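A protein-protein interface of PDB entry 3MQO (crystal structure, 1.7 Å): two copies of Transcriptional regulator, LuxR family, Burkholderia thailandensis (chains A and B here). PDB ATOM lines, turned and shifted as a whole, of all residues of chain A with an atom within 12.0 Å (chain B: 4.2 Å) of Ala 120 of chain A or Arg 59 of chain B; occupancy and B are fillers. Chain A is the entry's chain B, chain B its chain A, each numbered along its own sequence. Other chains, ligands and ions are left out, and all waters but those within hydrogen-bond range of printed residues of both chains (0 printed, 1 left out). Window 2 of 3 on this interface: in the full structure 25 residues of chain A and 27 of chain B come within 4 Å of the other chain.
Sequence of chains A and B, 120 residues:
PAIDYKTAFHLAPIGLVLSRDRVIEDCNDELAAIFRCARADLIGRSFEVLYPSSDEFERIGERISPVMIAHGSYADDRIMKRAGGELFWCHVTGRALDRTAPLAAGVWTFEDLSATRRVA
No position is printed for both chains.
NH2 of Arg 59 of chain B is in hydrogen-bond range of O of Ala 120 of chain A (3.5 Å). The guanidinium group (NH1) of Arg 117 of chain A is in salt-bridge range of the side-chain carboxylate (OD1) of Asp 77 of chain B (2.9 Å). The backbone NH (N) of Asp 77 of chain B lies within hydrogen-bond range of the backbone carbonyl oxygen (O) of Arg 118 of chain A, at 2.9 Å. N of Ala 120 of chain A is in hydrogen-bond range of O of Asp 77 of chain B, 3.1 Å away.
Thr 116 of chain A touches none of the printed residues of chain B. Of the printed residues of chain B, Arg 117 of chain A touches Asp 77. Printed residues of chain B within 4 Å of Arg 118 of chain A: Asp 76 and Asp 77. Of the printed residues of chain B, Val 119 of chain A touches Asp 77 (3.6 Å). Of the printed residues of chain B, Ala 120 of chain A touches Arg 59 (3.5 Å), Ile 60 (3.997 Å), Asp 76 (3.2 Å), Asp 77 (3.1 Å) and Arg 78 (3.96 Å). No residue of chain A comes within 4 Å of Asp 55 of chain B. Phe 57 of chain B touches none of the printed residues of chain A. No residue of chain A comes within 4 Å of Glu 58 of chain B. Arg 59 of chain B touches one residue of chain A. Of the printed residues of chain A, Ile 60 of chain B touches Ala 120. Of chain A, only Arg 117 (2.9 Å), Arg 118 (2.9 Å), Val 119 (3.6 Å) and Ala 120 (3.1 Å) come within 4 Å of Asp 77 of chain B. Arg 78 of chain B touches just one residue of chain A: Ala 120 (3.96 Å).
Hydrophobic or aromatic side chains of chain B within 4 Å of the printed part of chain A: Ile 60. Among the printed residues, 9 pairs touch across the chains.
The side-chain carboxylate (OE2) of Glu 56 of chain B lies within salt-bridge range of the guanidinium group (NE) of Arg 59 of chain B. The side-chain carboxylate (OD1) of Asp 76 of chain B is in salt-bridge range of the guanidinium group (NE) of Arg 78 of chain B (2.7 Å).
Among the printed residues, pairs that only touch across the chains: Arg 118 of chain A with Asp 76 of chain B (3.0 Å), Val 119 of chain A with Asp 77 of chain B (3.6 Å), Ala 120 of chain A with Ile 60 of chain B (3.997 Å), Ala 120 of chain A with Asp 76 of chain B (3.2 Å) and Ala 120 of chain A with Arg 78 of chain B (3.96 Å).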
ATOM      1  N   THR A 116      -4.040 -15.694  11.866  1.00  0.00           N
ATOM      2  CA  THR A 116      -5.482 -15.921  11.742  1.00  0.00           C
ATOM      3  C   THR A 116      -5.853 -17.187  12.511  1.00  0.00           C
ATOM      4  O   THR A 116      -5.182 -18.214  12.377  1.00  0.00           O
ATOM      5  CB  THR A 116      -5.904 -16.067  10.255  1.00  0.00           C
ATOM      6  OG1 THR A 116      -5.466 -14.918   9.519  1.00  0.00           O
ATOM      7  CG2 THR A 116      -7.432 -16.199  10.107  1.00  0.00           C
ATOM      8  N   ARG A 117      -6.902 -17.104  13.328  1.00  0.00           N
ATOM      9  CA  ARG A 117      -7.345 -18.272  14.091  1.00  0.00           C
ATOM     10  C   ARG A 117      -8.005 -19.283  13.175  1.00  0.00           C
ATOM     11  O   ARG A 117      -8.943 -18.953  12.440  1.00  0.00           O
ATOM     12  CB  ARG A 117      -8.283 -17.877  15.236  1.00  0.00           C
ATOM     13  CG  ARG A 117      -7.576 -17.162  16.379  1.00  0.00           C
ATOM     14  CD  ARG A 117      -8.553 -16.723  17.475  1.00  0.00           C
ATOM     15  NE  ARG A 117      -8.811 -17.779  18.458  1.00  0.00           N
ATOM     16  CZ  ARG A 117      -8.077 -18.000  19.549  1.00  0.00           C
ATOM     17  NH1 ARG A 117      -8.406 -18.981  20.373  1.00  0.00           N
ATOM     18  NH2 ARG A 117      -7.021 -17.241  19.824  1.00  0.00           N
ATOM     19  N   ARG A 118      -7.489 -20.508  13.203  1.00  0.00           N
ATOM     20  CA  ARG A 118      -8.091 -21.619  12.479  1.00  0.00           C
ATOM     21  C   ARG A 118      -9.282 -22.125  13.273  1.00  0.00           C
ATOM     22  O   ARG A 118      -9.161 -22.399  14.462  1.00  0.00           O
ATOM     23  CB  ARG A 118      -7.077 -22.758  12.299  1.00  0.00           C
ATOM     24  N   VAL A 119     -10.435 -22.228  12.623  1.00  0.00           N
ATOM     25  CA  VAL A 119     -11.590 -22.865  13.240  1.00  0.00           C
ATOM     26  C   VAL A 119     -11.772 -24.212  12.544  1.00  0.00           C
ATOM     27  O   VAL A 119     -12.073 -24.262  11.351  1.00  0.00           O
ATOM     28  CB  VAL A 119     -12.869 -21.982  13.153  1.00  0.00           C
ATOM     29  CG1 VAL A 119     -14.027 -22.637  13.898  1.00  0.00           C
ATOM     30  CG2 VAL A 119     -12.598 -20.591  13.729  1.00  0.00           C
ATOM     31  N   ALA A 120     -11.561 -25.290  13.300  1.00  0.00           N
ATOM     32  CA  ALA A 120     -11.498 -26.660  12.759  1.00  0.00           C
ATOM     33  C   ALA A 120     -12.731 -27.034  11.941  1.00  0.00           C
ATOM     34  O   ALA A 120     -13.861 -26.792  12.364  1.00  0.00           O
ATOM     35  CB  ALA A 120     -11.294 -27.658  13.876  1.00  0.00           C
ATOM     36  N   ASP B  55     -17.206 -39.273  14.818  1.00  0.00           N
ATOM     37  CA  ASP B  55     -17.016 -38.625  13.513  1.00  0.00           C
ATOM     38  C   ASP B  55     -16.199 -37.328  13.618  1.00  0.00           C
ATOM     39  O   ASP B  55     -15.379 -37.022  12.751  1.00  0.00           O
ATOM     40  CB  ASP B  55     -18.363 -38.349  12.835  1.00  0.00           C
ATOM     41  CG  ASP B  55     -19.045 -39.618  12.336  1.00  0.00           C
ATOM     42  OD1 ASP B  55     -18.450 -40.716  12.456  1.00  0.00           O
ATOM     43  OD2 ASP B  55     -20.179 -39.512  11.827  1.00  0.00           O
ATOM     44  N   GLU B  56     -16.440 -36.562  14.677  1.00  0.00           N
ATOM     45  CA  GLU B  56     -15.699 -35.314  14.906  1.00  0.00           C
ATOM     46  C   GLU B  56     -14.229 -35.566  15.221  1.00  0.00           C
ATOM     47  O   GLU B  56     -13.349 -34.876  14.715  1.00  0.00           O
ATOM     48  CB  GLU B  56     -16.382 -34.468  15.983  1.00  0.00           C
ATOM     49  CG  GLU B  56     -17.592 -33.694  15.444  1.00  0.00           C
ATOM     50  CD  GLU B  56     -17.194 -32.659  14.413  1.00  0.00           C
ATOM     51  OE1 GLU B  56     -16.793 -31.538  14.805  1.00  0.00           O
ATOM     52  OE2 GLU B  56     -17.270 -32.969  13.206  1.00  0.00           O
ATOM     53  N   PHE B  57     -13.981 -36.589  16.033  1.00  0.00           N
ATOM     54  CA  PHE B  57     -12.634 -37.055  16.357  1.00  0.00           C
ATOM     55  C   PHE B  57     -11.894 -37.446  15.064  1.00  0.00           C
ATOM     56  O   PHE B  57     -10.735 -37.082  14.875  1.00  0.00           O
ATOM     57  CB  PHE B  57     -12.759 -38.242  17.316  1.00  0.00           C
ATOM     58  CG  PHE B  57     -11.512 -39.070  17.455  1.00  0.00           C
ATOM     59  CD1 PHE B  57     -10.423 -38.593  18.181  1.00  0.00           C
ATOM     60  CD2 PHE B  57     -11.438 -40.347  16.881  1.00  0.00           C
ATOM     61  CE1 PHE B  57      -9.296 -39.366  18.350  1.00  0.00           C
ATOM     62  CE2 PHE B  57     -10.290 -41.138  17.028  1.00  0.00           C
ATOM     63  CZ  PHE B  57      -9.214 -40.649  17.769  1.00  0.00           C
ATOM     64  N   GLU B  58     -12.594 -38.135  14.156  1.00  0.00           N
ATOM     65  CA  GLU B  58     -12.019 -38.497  12.852  1.00  0.00           C
ATOM     66  C   GLU B  58     -11.771 -37.289  11.948  1.00  0.00           C
ATOM     67  O   GLU B  58     -10.692 -37.155  11.373  1.00  0.00           O
ATOM     68  CB  GLU B  58     -12.919 -39.504  12.124  1.00  0.00           C
ATOM     69  CG  GLU B  58     -13.027 -40.850  12.831  1.00  0.00           C
ATOM     70  CD  GLU B  58     -11.709 -41.601  12.883  1.00  0.00           C
ATOM     71  OE1 GLU B  58     -10.857 -41.391  11.992  1.00  0.00           O
ATOM     72  OE2 GLU B  58     -11.530 -42.420  13.811  1.00  0.00           O
ATOM     73  N   ARG B  59     -12.783 -36.431  11.815  1.00  0.00           N
ATOM     74  CA  ARG B  59     -12.740 -35.272  10.934  1.00  0.00           C
ATOM     75  C   ARG B  59     -11.622 -34.334  11.331  1.00  0.00           C
ATOM     76  O   ARG B  59     -10.860 -33.866  10.490  1.00  0.00           O
ATOM     77  CB  ARG B  59     -14.068 -34.508  10.987  1.00  0.00           C
ATOM     78  CG  ARG B  59     -14.193 -33.413   9.926  1.00  0.00           C
ATOM     79  CD  ARG B  59     -15.506 -32.636  10.069  1.00  0.00           C
ATOM     80  NE  ARG B  59     -15.552 -31.841  11.303  1.00  0.00           N
ATOM     81  CZ  ARG B  59     -14.996 -30.639  11.463  1.00  0.00           C
ATOM     82  NH1 ARG B  59     -14.315 -30.061  10.478  1.00  0.00           N
ATOM     83  NH2 ARG B  59     -15.112 -30.011  12.628  1.00  0.00           N
ATOM     84  N   ILE B  60     -11.537 -34.050  12.622  1.00  0.00           N
ATOM     85  CA  ILE B  60     -10.540 -33.114  13.098  1.00  0.00           C
ATOM     86  C   ILE B  60      -9.122 -33.714  13.043  1.00  0.00           C
ATOM     87  O   ILE B  60      -8.145 -32.996  12.838  1.00  0.00           O
ATOM     88  CB  ILE B  60     -10.953 -32.500  14.473  1.00  0.00           C
ATOM     89  CG1 ILE B  60     -12.142 -31.546  14.248  1.00  0.00           C
ATOM     90  CG2 ILE B  60      -9.802 -31.751  15.137  1.00  0.00           C
ATOM     91  CD1 ILE B  60     -12.894 -31.145  15.507  1.00  0.00           C
ATOM     92  N   GLY B  61      -9.012 -35.029  13.211  1.00  0.00           N
ATOM     93  CA  GLY B  61      -7.718 -35.697  13.037  1.00  0.00           C
ATOM     94  C   GLY B  61      -7.189 -35.476  11.626  1.00  0.00           C
ATOM     95  O   GLY B  61      -6.001 -35.229  11.430  1.00  0.00           O
ATOM     96  N   GLU B  62      -8.082 -35.568  10.637  1.00  0.00           N
ATOM     97  CA  GLU B  62      -7.715 -35.361   9.234  1.00  0.00           C
ATOM     98  C   GLU B  62      -7.382 -33.894   8.922  1.00  0.00           C
ATOM     99  O   GLU B  62      -6.631 -33.622   7.993  1.00  0.00           O
ATOM    100  CB  GLU B  62      -8.809 -35.901   8.300  1.00  0.00           C
ATOM    101  CG  GLU B  62      -8.902 -37.430   8.321  1.00  0.00           C
ATOM    102  CD  GLU B  62      -9.950 -37.991   7.375  1.00  0.00           C
ATOM    103  OE1 GLU B  62     -11.124 -37.566   7.445  1.00  0.00           O
ATOM    104  OE2 GLU B  62      -9.603 -38.883   6.573  1.00  0.00           O
ATOM    105  N   ARG B  63      -7.950 -32.962   9.687  1.00  0.00           N
ATOM    106  CA  ARG B  63      -7.616 -31.535   9.568  1.00  0.00           C
ATOM    107  C   ARG B  63      -6.260 -31.236  10.207  1.00  0.00           C
ATOM    108  O   ARG B  63      -5.487 -30.413   9.693  1.00  0.00           O
ATOM    109  CB  ARG B  63      -8.698 -30.657  10.204  1.00  0.00           C
ATOM    110  N   ASP B  76      -6.170 -24.553  16.750  1.00  0.00           N
ATOM    111  CA  ASP B  76      -7.509 -24.272  16.209  1.00  0.00           C
ATOM    112  C   ASP B  76      -8.469 -23.964  17.340  1.00  0.00           C
ATOM    113  O   ASP B  76      -8.074 -23.968  18.489  1.00  0.00           O
ATOM    114  CB  ASP B  76      -8.028 -25.434  15.342  1.00  0.00           C
ATOM    115  CG  ASP B  76      -8.489 -26.611  16.147  1.00  0.00           C
ATOM    116  OD1 ASP B  76      -8.829 -26.428  17.332  1.00  0.00           O
ATOM    117  OD2 ASP B  76      -8.549 -27.720  15.579  1.00  0.00           O
ATOM    118  N   ASP B  77      -9.718 -23.673  16.999  1.00  0.00           N
ATOM    119  CA  ASP B  77     -10.774 -23.646  17.984  1.00  0.00           C
ATOM    120  C   ASP B  77     -11.766 -24.668  17.509  1.00  0.00           C
ATOM    121  O   ASP B  77     -11.982 -24.786  16.304  1.00  0.00           O
ATOM    122  CB  ASP B  77     -11.407 -22.253  18.030  1.00  0.00           C
ATOM    123  CG  ASP B  77     -10.403 -21.189  18.396  1.00  0.00           C
ATOM    124  OD1 ASP B  77      -9.726 -21.350  19.454  1.00  0.00           O
ATOM    125  OD2 ASP B  77     -10.251 -20.227  17.609  1.00  0.00           O
ATOM    126  N   ARG B  78     -12.338 -25.431  18.439  1.00  0.00           N
ATOM    127  CA  ARG B  78     -13.387 -26.402  18.084  1.00  0.00           C
ATOM    128  C   ARG B  78     -14.319 -26.666  19.242  1.00  0.00           C
ATOM    129  O   ARG B  78     -13.978 -26.415  20.398  1.00  0.00           O
ATOM    130  CB  ARG B  78     -12.810 -27.719  17.539  1.00  0.00           C
ATOM    131  CG  ARG B  78     -12.472 -28.747  18.601  1.00  0.00           C
ATOM    132  CD  ARG B  78     -11.186 -28.341  19.342  1.00  0.00           C
ATOM    133  NE  ARG B  78      -9.997 -28.590  18.525  1.00  0.00           N
ATOM    134  CZ  ARG B  78      -9.347 -29.754  18.476  1.00  0.00           C
ATOM    135  NH1 ARG B  78      -9.776 -30.797  19.186  1.00  0.00           N
ATOM    136  NH2 ARG B  78      -8.280 -29.876  17.705  1.00  0.00           N
